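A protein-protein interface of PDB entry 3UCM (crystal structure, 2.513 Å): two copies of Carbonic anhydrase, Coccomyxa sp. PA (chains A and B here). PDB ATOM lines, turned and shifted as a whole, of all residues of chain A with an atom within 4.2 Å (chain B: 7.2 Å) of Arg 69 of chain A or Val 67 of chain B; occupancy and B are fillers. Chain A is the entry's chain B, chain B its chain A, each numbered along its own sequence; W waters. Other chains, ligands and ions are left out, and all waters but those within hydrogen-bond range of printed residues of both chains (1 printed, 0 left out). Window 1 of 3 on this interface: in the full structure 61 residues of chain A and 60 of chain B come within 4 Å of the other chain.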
ATOM      1  N   GLY A  46     -16.294 -27.880  -3.961  1.00  0.00           N
ATOM      2  CA  GLY A  46     -16.425 -29.292  -4.436  1.00  0.00           C
ATOM      3  C   GLY A  46     -17.241 -29.565  -5.687  1.00  0.00           C
ATOM      4  O   GLY A  46     -17.801 -28.657  -6.272  1.00  0.00           O
ATOM      5  N   CYS A  47     -17.364 -30.826  -6.091  1.00  0.00           N
ATOM      6  CA  CYS A  47     -18.164 -31.150  -7.276  1.00  0.00           C
ATOM      7  C   CYS A  47     -19.663 -31.189  -6.964  1.00  0.00           C
ATOM      8  O   CYS A  47     -20.118 -31.420  -5.799  1.00  0.00           O
ATOM      9  CB  CYS A  47     -17.715 -32.447  -7.986  1.00  0.00           C
ATOM     10  SG  CYS A  47     -18.372 -32.656  -9.748  1.00  0.00           S
ATOM     11  N   ALA A  48     -20.420 -30.918  -8.017  1.00  0.00           N
ATOM     12  CA  ALA A  48     -21.862 -30.907  -7.958  1.00  0.00           C
ATOM     13  C   ALA A  48     -22.553 -32.303  -7.958  1.00  0.00           C
ATOM     14  O   ALA A  48     -23.749 -32.358  -7.768  1.00  0.00           O
ATOM     15  CB  ALA A  48     -22.378 -30.046  -9.112  1.00  0.00           C
ATOM     16  N   ASP A  49     -21.798 -33.383  -8.200  1.00  0.00           N
ATOM     17  CA  ASP A  49     -22.262 -34.787  -8.365  1.00  0.00           C
ATOM     18  C   ASP A  49     -23.055 -35.251  -7.151  1.00  0.00           C
ATOM     19  O   ASP A  49     -22.658 -34.976  -6.017  1.00  0.00           O
ATOM     20  CB  ASP A  49     -21.005 -35.660  -8.545  1.00  0.00           C
ATOM     21  CG  ASP A  49     -21.286 -37.141  -8.821  1.00  0.00           C
ATOM     22  OD1 ASP A  49     -20.929 -37.635  -9.927  1.00  0.00           O
ATOM     23  OD2 ASP A  49     -21.774 -37.839  -7.903  1.00  0.00           O
ATOM     24  N   VAL A  52     -21.478 -36.814  -3.471  1.00  0.00           N
ATOM     25  CA  VAL A  52     -20.424 -36.165  -2.671  1.00  0.00           C
ATOM     26  C   VAL A  52     -21.007 -35.002  -1.840  1.00  0.00           C
ATOM     27  O   VAL A  52     -20.987 -33.838  -2.297  1.00  0.00           O
ATOM     28  CB  VAL A  52     -19.236 -35.653  -3.603  1.00  0.00           C
ATOM     29  CG1 VAL A  52     -17.979 -35.249  -2.798  1.00  0.00           C
ATOM     30  CG2 VAL A  52     -18.863 -36.694  -4.700  1.00  0.00           C
ATOM     31  N   SER A  53     -21.558 -35.311  -0.658  1.00  0.00           N
ATOM     32  CA  SER A  53     -22.310 -34.342   0.139  1.00  0.00           C
ATOM     33  C   SER A  53     -21.477 -33.816   1.343  1.00  0.00           C
ATOM     34  O   SER A  53     -21.437 -34.460   2.398  1.00  0.00           O
ATOM     35  CB  SER A  53     -23.630 -34.970   0.645  1.00  0.00           C
ATOM     36  OG  SER A  53     -24.584 -35.247  -0.381  1.00  0.00           O
ATOM     37  N   PRO A  54     -20.815 -32.642   1.216  1.00  0.00           N
ATOM     38  CA  PRO A  54     -19.766 -32.401   2.243  1.00  0.00           C
ATOM     39  C   PRO A  54     -20.220 -32.346   3.707  1.00  0.00           C
ATOM     40  O   PRO A  54     -19.590 -32.964   4.562  1.00  0.00           O
ATOM     41  CB  PRO A  54     -19.126 -31.090   1.808  1.00  0.00           C
ATOM     42  CG  PRO A  54     -20.211 -30.412   0.981  1.00  0.00           C
ATOM     43  CD  PRO A  54     -20.886 -31.540   0.240  1.00  0.00           C
ATOM     44  N   VAL A  67     -20.103 -23.616   1.676  1.00  0.00           N
ATOM     45  CA  VAL A  67     -19.964 -24.492   0.478  1.00  0.00           C
ATOM     46  C   VAL A  67     -20.088 -23.833  -0.905  1.00  0.00           C
ATOM     47  O   VAL A  67     -21.057 -23.155  -1.143  1.00  0.00           O
ATOM     48  CB  VAL A  67     -21.006 -25.698   0.540  1.00  0.00           C
ATOM     49  CG1 VAL A  67     -20.967 -26.597  -0.755  1.00  0.00           C
ATOM     50  CG2 VAL A  67     -20.820 -26.567   1.838  1.00  0.00           C
ATOM     51  N   GLN A  68     -19.129 -24.080  -1.813  1.00  0.00           N
ATOM     52  CA  GLN A  68     -19.302 -23.931  -3.268  1.00  0.00           C
ATOM     53  C   GLN A  68     -19.332 -25.290  -4.011  1.00  0.00           C
ATOM     54  O   GLN A  68     -18.508 -26.174  -3.781  1.00  0.00           O
ATOM     55  CB  GLN A  68     -18.196 -23.050  -3.847  1.00  0.00           C
ATOM     56  CG  GLN A  68     -17.916 -23.210  -5.343  1.00  0.00           C
ATOM     57  CD  GLN A  68     -18.851 -22.455  -6.286  1.00  0.00           C
ATOM     58  OE1 GLN A  68     -18.688 -22.570  -7.496  1.00  0.00           O
ATOM     59  NE2 GLN A  68     -19.817 -21.658  -5.750  1.00  0.00           N
ATOM     60  N   ARG A  69     -20.265 -25.470  -4.926  1.00  0.00           N
ATOM     61  CA  ARG A  69     -20.401 -26.770  -5.627  1.00  0.00           C
ATOM     62  C   ARG A  69     -20.729 -26.507  -7.108  1.00  0.00           C
ATOM     63  O   ARG A  69     -21.745 -25.857  -7.395  1.00  0.00           O
ATOM     64  CB  ARG A  69     -21.453 -27.687  -4.924  1.00  0.00           C
ATOM     65  CG  ARG A  69     -20.845 -28.605  -3.778  1.00  0.00           C
ATOM     66  CD  ARG A  69     -21.851 -29.563  -3.036  1.00  0.00           C
ATOM     67  NE  ARG A  69     -22.117 -30.757  -3.858  1.00  0.00           N
ATOM     68  CZ  ARG A  69     -23.034 -31.688  -3.601  1.00  0.00           C
ATOM     69  NH1 ARG A  69     -23.804 -31.640  -2.529  1.00  0.00           N
ATOM     70  NH2 ARG A  69     -23.196 -32.677  -4.442  1.00  0.00           N
ATOM     71  N   ASN A  70     -19.849 -26.947  -8.019  1.00  0.00           N
ATOM     72  CA  ASN A  70     -20.046 -26.716  -9.438  1.00  0.00           C
ATOM     73  C   ASN A  70     -19.580 -27.916 -10.225  1.00  0.00           C
ATOM     74  O   ASN A  70     -18.825 -28.673  -9.696  1.00  0.00           O
ATOM     75  CB  ASN A  70     -19.296 -25.454  -9.885  1.00  0.00           C
ATOM     76  CG  ASN A  70     -17.804 -25.657  -9.969  1.00  0.00           C
ATOM     77  OD1 ASN A  70     -17.315 -26.514 -10.730  1.00  0.00           O
ATOM     78  ND2 ASN A  70     -17.063 -24.883  -9.182  1.00  0.00           N
ATOM     79  N   TYR B  42     -33.602 -35.598  -8.192  1.00  0.00           N
ATOM     80  CA  TYR B  42     -33.582 -34.195  -7.775  1.00  0.00           C
ATOM     81  C   TYR B  42     -32.304 -33.368  -8.113  1.00  0.00           C
ATOM     82  O   TYR B  42     -31.178 -33.846  -7.910  1.00  0.00           O
ATOM     83  CB  TYR B  42     -33.782 -34.122  -6.251  1.00  0.00           C
ATOM     84  CG  TYR B  42     -35.123 -34.628  -5.761  1.00  0.00           C
ATOM     85  CD1 TYR B  42     -36.216 -33.767  -5.672  1.00  0.00           C
ATOM     86  CD2 TYR B  42     -35.311 -35.980  -5.418  1.00  0.00           C
ATOM     87  CE1 TYR B  42     -37.487 -34.217  -5.212  1.00  0.00           C
ATOM     88  CE2 TYR B  42     -36.575 -36.457  -4.978  1.00  0.00           C
ATOM     89  CZ  TYR B  42     -37.664 -35.567  -4.874  1.00  0.00           C
ATOM     90  OH  TYR B  42     -38.890 -35.995  -4.404  1.00  0.00           O
ATOM     91  N   LEU B  43     -32.509 -32.137  -8.618  1.00  0.00           N
ATOM     92  CA  LEU B  43     -31.514 -31.044  -8.571  1.00  0.00           C
ATOM     93  C   LEU B  43     -31.904 -30.042  -7.486  1.00  0.00           C
ATOM     94  O   LEU B  43     -33.062 -29.702  -7.407  1.00  0.00           O
ATOM     95  CB  LEU B  43     -31.425 -30.297  -9.918  1.00  0.00           C
ATOM     96  CG  LEU B  43     -30.672 -28.943  -9.927  1.00  0.00           C
ATOM     97  CD1 LEU B  43     -29.218 -29.087  -9.569  1.00  0.00           C
ATOM     98  CD2 LEU B  43     -30.762 -28.153 -11.261  1.00  0.00           C
ATOM     99  N   TYR B  44     -30.959 -29.556  -6.671  1.00  0.00           N
ATOM    100  CA  TYR B  44     -31.250 -28.540  -5.639  1.00  0.00           C
ATOM    101  C   TYR B  44     -30.359 -27.333  -5.877  1.00  0.00           C
ATOM    102  O   TYR B  44     -29.137 -27.500  -6.050  1.00  0.00           O
ATOM    103  CB  TYR B  44     -30.933 -29.102  -4.287  1.00  0.00           C
ATOM    104  CG  TYR B  44     -30.757 -28.120  -3.126  1.00  0.00           C
ATOM    105  CD1 TYR B  44     -31.818 -27.864  -2.243  1.00  0.00           C
ATOM    106  CD2 TYR B  44     -29.506 -27.533  -2.837  1.00  0.00           C
ATOM    107  CE1 TYR B  44     -31.675 -27.038  -1.161  1.00  0.00           C
ATOM    108  CE2 TYR B  44     -29.346 -26.672  -1.724  1.00  0.00           C
ATOM    109  CZ  TYR B  44     -30.450 -26.448  -0.884  1.00  0.00           C
ATOM    110  OH  TYR B  44     -30.372 -25.601   0.199  1.00  0.00           O
ATOM    111  N   ILE B  45     -30.952 -26.126  -5.907  1.00  0.00           N
ATOM    112  CA  ILE B  45     -30.211 -24.867  -6.095  1.00  0.00           C
ATOM    113  C   ILE B  45     -30.410 -24.019  -4.834  1.00  0.00           C
ATOM    114  O   ILE B  45     -31.519 -23.677  -4.506  1.00  0.00           O
ATOM    115  CB  ILE B  45     -30.699 -24.098  -7.347  1.00  0.00           C
ATOM    116  CG1 ILE B  45     -30.300 -24.816  -8.663  1.00  0.00           C
ATOM    117  CG2 ILE B  45     -30.182 -22.641  -7.345  1.00  0.00           C
ATOM    118  CD1 ILE B  45     -31.078 -24.286  -9.864  1.00  0.00           C
ATOM    119  N   GLY B  46     -29.344 -23.704  -4.110  1.00  0.00           N
ATOM    120  CA  GLY B  46     -29.511 -23.099  -2.773  1.00  0.00           C
ATOM    121  C   GLY B  46     -28.325 -22.247  -2.336  1.00  0.00           C
ATOM    122  O   GLY B  46     -27.408 -21.986  -3.150  1.00  0.00           O
ATOM    123  N   ALA B  48     -24.917 -20.851  -0.407  1.00  0.00           N
ATOM    124  CA  ALA B  48     -23.611 -21.281   0.156  1.00  0.00           C
ATOM    125  C   ALA B  48     -23.445 -21.127   1.704  1.00  0.00           C
ATOM    126  O   ALA B  48     -22.455 -21.636   2.283  1.00  0.00           O
ATOM    127  CB  ALA B  48     -22.499 -20.487  -0.459  1.00  0.00           C
ATOM    128  N   PRO B  54     -28.181 -29.300   2.248  1.00  0.00           N
ATOM    129  CA  PRO B  54     -29.295 -30.015   1.587  1.00  0.00           C
ATOM    130  C   PRO B  54     -29.419 -31.495   1.947  1.00  0.00           C
ATOM    131  O   PRO B  54     -30.464 -31.931   2.462  1.00  0.00           O
ATOM    132  CB  PRO B  54     -28.973 -29.902   0.109  1.00  0.00           C
ATOM    133  CG  PRO B  54     -27.636 -29.090  -0.030  1.00  0.00           C
ATOM    134  CD  PRO B  54     -27.392 -28.469   1.312  1.00  0.00           C
ATOM    135  N   ALA B  55     -28.371 -32.268   1.687  1.00  0.00           N
ATOM    136  CA  ALA B  55     -28.404 -33.681   1.954  1.00  0.00           C
ATOM    137  C   ALA B  55     -28.755 -34.032   3.404  1.00  0.00           C
ATOM    138  O   ALA B  55     -29.469 -34.999   3.656  1.00  0.00           O
ATOM    139  CB  ALA B  55     -27.115 -34.327   1.550  1.00  0.00           C
ATOM    140  N   VAL B  65     -29.503 -36.398  -4.645  1.00  0.00           N
ATOM    141  CA  VAL B  65     -29.641 -34.968  -4.955  1.00  0.00           C
ATOM    142  C   VAL B  65     -28.323 -34.354  -5.448  1.00  0.00           C
ATOM    143  O   VAL B  65     -27.324 -34.304  -4.718  1.00  0.00           O
ATOM    144  CB  VAL B  65     -30.257 -34.197  -3.768  1.00  0.00           C
ATOM    145  CG1 VAL B  65     -29.305 -34.197  -2.570  1.00  0.00           C
ATOM    146  CG2 VAL B  65     -30.658 -32.768  -4.176  1.00  0.00           C
ATOM    147  N   PHE B  66     -28.339 -33.958  -6.719  1.00  0.00           N
ATOM    148  CA  PHE B  66     -27.313 -33.152  -7.394  1.00  0.00           C
ATOM    149  C   PHE B  66     -27.582 -31.702  -6.920  1.00  0.00           C
ATOM    150  O   PHE B  66     -28.771 -31.231  -6.904  1.00  0.00           O
ATOM    151  CB  PHE B  66     -27.572 -33.289  -8.893  1.00  0.00           C
ATOM    152  CG  PHE B  66     -26.439 -32.819  -9.824  1.00  0.00           C
ATOM    153  CD1 PHE B  66     -25.647 -33.777 -10.546  1.00  0.00           C
ATOM    154  CD2 PHE B  66     -26.220 -31.452 -10.058  1.00  0.00           C
ATOM    155  CE1 PHE B  66     -24.666 -33.362 -11.489  1.00  0.00           C
ATOM    156  CE2 PHE B  66     -25.208 -31.016 -10.996  1.00  0.00           C
ATOM    157  CZ  PHE B  66     -24.437 -31.954 -11.706  1.00  0.00           C
ATOM    158  N   VAL B  67     -26.500 -31.017  -6.522  1.00  0.00           N
ATOM    159  CA  VAL B  67     -26.562 -29.709  -5.854  1.00  0.00           C
ATOM    160  C   VAL B  67     -25.704 -28.566  -6.503  1.00  0.00           C
ATOM    161  O   VAL B  67     -24.497 -28.720  -6.728  1.00  0.00           O
ATOM    162  CB  VAL B  67     -26.107 -29.901  -4.403  1.00  0.00           C
ATOM    163  CG1 VAL B  67     -25.662 -28.547  -3.730  1.00  0.00           C
ATOM    164  CG2 VAL B  67     -27.166 -30.667  -3.605  1.00  0.00           C
ATOM    165  N   GLN B  68     -26.327 -27.413  -6.780  1.00  0.00           N
ATOM    166  CA  GLN B  68     -25.588 -26.146  -6.978  1.00  0.00           C
ATOM    167  C   GLN B  68     -25.777 -25.274  -5.751  1.00  0.00           C
ATOM    168  O   GLN B  68     -26.909 -25.152  -5.217  1.00  0.00           O
ATOM    169  CB  GLN B  68     -26.066 -25.425  -8.246  1.00  0.00           C
ATOM    170  CG  GLN B  68     -26.044 -23.892  -8.219  1.00  0.00           C
ATOM    171  CD  GLN B  68     -24.680 -23.239  -8.592  1.00  0.00           C
ATOM    172  OE1 GLN B  68     -24.564 -22.014  -8.595  1.00  0.00           O
ATOM    173  NE2 GLN B  68     -23.667 -24.055  -8.889  1.00  0.00           N
ATOM    174  N   ARG B  69     -24.683 -24.650  -5.312  1.00  0.00           N
ATOM    175  CA  ARG B  69     -24.703 -23.762  -4.149  1.00  0.00           C
ATOM    176  C   ARG B  69     -23.864 -22.464  -4.335  1.00  0.00           C
ATOM    177  O   ARG B  69     -22.655 -22.512  -4.638  1.00  0.00           O
ATOM    178  CB  ARG B  69     -24.298 -24.546  -2.892  1.00  0.00           C
ATOM    179  CG  ARG B  69     -25.492 -25.117  -2.153  1.00  0.00           C
ATOM    180  CD  ARG B  69     -25.078 -25.928  -0.938  1.00  0.00           C
ATOM    181  NE  ARG B  69     -24.967 -25.030   0.212  1.00  0.00           N
ATOM    182  CZ  ARG B  69     -24.460 -25.359   1.398  1.00  0.00           C
ATOM    183  NH1 ARG B  69     -24.001 -26.581   1.610  1.00  0.00           N
ATOM    184  NH2 ARG B  69     -24.439 -24.458   2.382  1.00  0.00           N
ATOM    185  N   ASN B  70     -24.524 -21.298  -4.192  1.00  0.00           N
ATOM    186  CA  ASN B  70     -23.880 -19.996  -4.421  1.00  0.00           C
ATOM    187  C   ASN B  70     -24.415 -18.911  -3.459  1.00  0.00           C
ATOM    188  O   ASN B  70     -25.469 -19.122  -2.807  1.00  0.00           O
ATOM    189  CB  ASN B  70     -23.979 -19.613  -5.910  1.00  0.00           C
ATOM    190  CG  ASN B  70     -25.361 -19.196  -6.307  1.00  0.00           C
ATOM    191  OD1 ASN B  70     -25.843 -18.180  -5.833  1.00  0.00           O
ATOM    192  ND2 ASN B  70     -26.015 -19.952  -7.210  1.00  0.00           N
ATOM    193  N   ASN B  81     -21.774 -21.203 -14.593  1.00  0.00           N
ATOM    194  CA  ASN B  81     -21.593 -22.082 -13.416  1.00  0.00           C
ATOM    195  C   ASN B  81     -22.960 -22.724 -13.101  1.00  0.00           C
ATOM    196  O   ASN B  81     -23.107 -23.914 -13.185  1.00  0.00           O
ATOM    197  CB  ASN B  81     -21.091 -21.220 -12.226  1.00  0.00           C
ATOM    198  CG  ASN B  81     -20.616 -22.014 -11.010  1.00  0.00           C
ATOM    199  OD1 ASN B  81     -21.314 -22.861 -10.469  1.00  0.00           O
ATOM    200  ND2 ASN B  81     -19.441 -21.668 -10.526  1.00  0.00           N
ATOM    201  N   CYS B  82     -23.949 -21.930 -12.720  1.00  0.00           N
ATOM    202  CA  CYS B  82     -25.257 -22.446 -12.403  1.00  0.00           C
ATOM    203  C   CYS B  82     -25.923 -23.092 -13.656  1.00  0.00           C
ATOM    204  O   CYS B  82     -26.534 -24.140 -13.570  1.00  0.00           O
ATOM    205  CB  CYS B  82     -26.142 -21.335 -11.774  1.00  0.00           C
ATOM    206  SG  CYS B  82     -27.745 -21.985 -11.288  1.00  0.00           S
ATOM    207  N   CYS B  85     -24.963 -26.802 -14.086  1.00  0.00           N
ATOM    208  CA  CYS B  85     -25.672 -27.719 -13.238  1.00  0.00           C
ATOM    209  C   CYS B  85     -27.079 -27.987 -13.824  1.00  0.00           C
ATOM    210  O   CYS B  85     -27.516 -29.108 -13.915  1.00  0.00           O
ATOM    211  CB  CYS B  85     -25.686 -27.183 -11.824  1.00  0.00           C
ATOM    212  SG  CYS B  85     -23.968 -27.010 -11.066  1.00  0.00           S
ATOM    213  N   THR B  89     -28.023 -31.949 -15.387  1.00  0.00           N
ATOM    214  CA  THR B  89     -29.154 -32.660 -14.772  1.00  0.00           C
ATOM    215  C   THR B  89     -30.359 -32.904 -15.710  1.00  0.00           C
ATOM    216  O   THR B  89     -30.864 -34.016 -15.781  1.00  0.00           O
ATOM    217  CB  THR B  89     -29.667 -31.995 -13.454  1.00  0.00           C
ATOM    218  OG1 THR B  89     -30.057 -30.628 -13.706  1.00  0.00           O
ATOM    219  CG2 THR B  89     -28.592 -32.068 -12.370  1.00  0.00           C
HETATM  220  O   HOH W   1     -25.567 -33.935  -2.846  1.00  0.00           O
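The backbone carbonyl oxygen (O) of Ala 48 of chain B lies within hydrogen-bond range of the backbone NH (N) of Val 67 of chain A, at 3.1 Å. NE2 of Gln 68 of chain A lies within hydrogen-bond range of O of Arg 69 of chain B (3.2 Å). The backbone NH (N) of Val 67 of chain B is in hydrogen-bond range of the backbone carbonyl oxygen (O) of Ala 48 of chain A (3.3 Å). NE2 of Gln 68 of chain B sits at hydrogen-bond distance from O of Arg 69 of chain A (3.0 Å). The side-chain amide oxygen (OE1) of Gln 68 of chain A is in hydrogen-bond range of the side-chain amide nitrogen (ND2) of Asn 81 of chain B, 3.2 Å away.
The side-chain amide nitrogen of Gln 68 of chain B is in hydrogen-bond range of the side-chain amide oxygen of Asn 81 of chain B, 3.1 Å away. O of Tyr 42 of chain B lies within hydrogen-bond range of N of Phe 66 of chain B, at 3.1 Å. O of Tyr 44 of chain B lies within hydrogen-bond range of N of Gln 68 of chain B, at 2.9 Å. The side-chain sulfur (SG) of Cys 85 of chain B is in hydrogen-bond range of the side-chain amide nitrogen (NE2) of Gln 68 of chain B (3.7 Å). The backbone carbonyl oxygen (O) of Val 52 of chain A sits close to the guanidinium group (NH2) of Arg 69 of chain A, at 3.3 Å. The backbone NH (N) of Tyr 44 of chain B lies within hydrogen-bond range of the backbone carbonyl oxygen (O) of Phe 66 of chain B (2.8 Å).
Among the printed residues, merely in contact across the chains: Val 67 of chain A with Arg 69 of chain B (3.2 Å), Ser 53 of chain A with Ala 55 of chain B (3.3 Å), Asn 70 of chain A with Asn 81 of chain B (3.3 Å), Ala 48 of chain A with Phe 66 of chain B (3.4 Å), Arg 69 of chain A with Val 67 of chain B (3.4 Å), Arg 69 of chain A with Arg 69 of chain B (3.8 Å) and Ala 48 of chain A with Cys 85 of chain B (3.9 Å).
Printed residues of chain B within 4 Å of Ala 48 of chain A: Phe 66 (3.4 Å), Val 67 (3.3 Å) and Cys 85 (3.9 Å). Of the printed residues of chain B, Val 67 of chain A touches Ala 48 (3.1 Å) and Arg 69 (3.2 Å). Tyr 42 of chain B touches none of the printed residues of chain A. Printed residues of chain A within 4 Å of Ala 55 of chain B: Ser 53 (3.3 Å). Of chain A, only Ala 48 (3.3 Å) and Arg 69 (3.4 Å) come within 4 Å of Val 67 of chain B. Of the printed residues of chain A, Arg 69 of chain B touches Val 67 (3.2 Å), Gln 68 (3.2 Å) and Arg 69 (3.8 Å). Printed residues of chain A within 4 Å of Cys 85 of chain B: Ala 48 (3.9 Å). The nearest printed residue of chain A that does not touch Arg 69 of chain B is Pro 54 of chain A (5.4 Å).
Of the 18 printed residues of chain B, 8 touch a printed residue of chain A. Along chain B the printed residues that touch a printed residue of chain A span positions 48 to 85. Printed residues of chain A that touch a printed residue of chain B: Ala 48, Ser 53, Val 67, Gln 68, Arg 69 and Asn 70. Hydrophobic or aromatic side chains of chain A that line the printed part of chain B: Ala 48 and Val 67. Among the printed residues, no Asp or Glu carboxylate lies within 4 Å of a Lys or Arg side-chain nitrogen of the other chain.
Ala 48 of chain A touches Val 67 of chain B, and with the chains exchanged Val 67 of chain A touches Ala 48 of chain B. Val 67 of chain A touches Arg 69 of chain B, and with the chains exchanged Arg 69 of chain A touches Val 67 of chain B. Gln 68 of chain A touches Arg 69 of chain B, and with the chains exchanged Arg 69 of chain A touches Gln 68 of chain B. Arg 69 of chain B touches its own counterpart, Arg 69 of chain A.
Water W1 lies within hydrogen-bond range of the backbone carbonyl oxygen (O) of Val 65 of chain B, the guanidinium group (NH1) of Arg 69 of chain A and the side-chain hydroxyl (OG) of Ser 53 of chain A.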
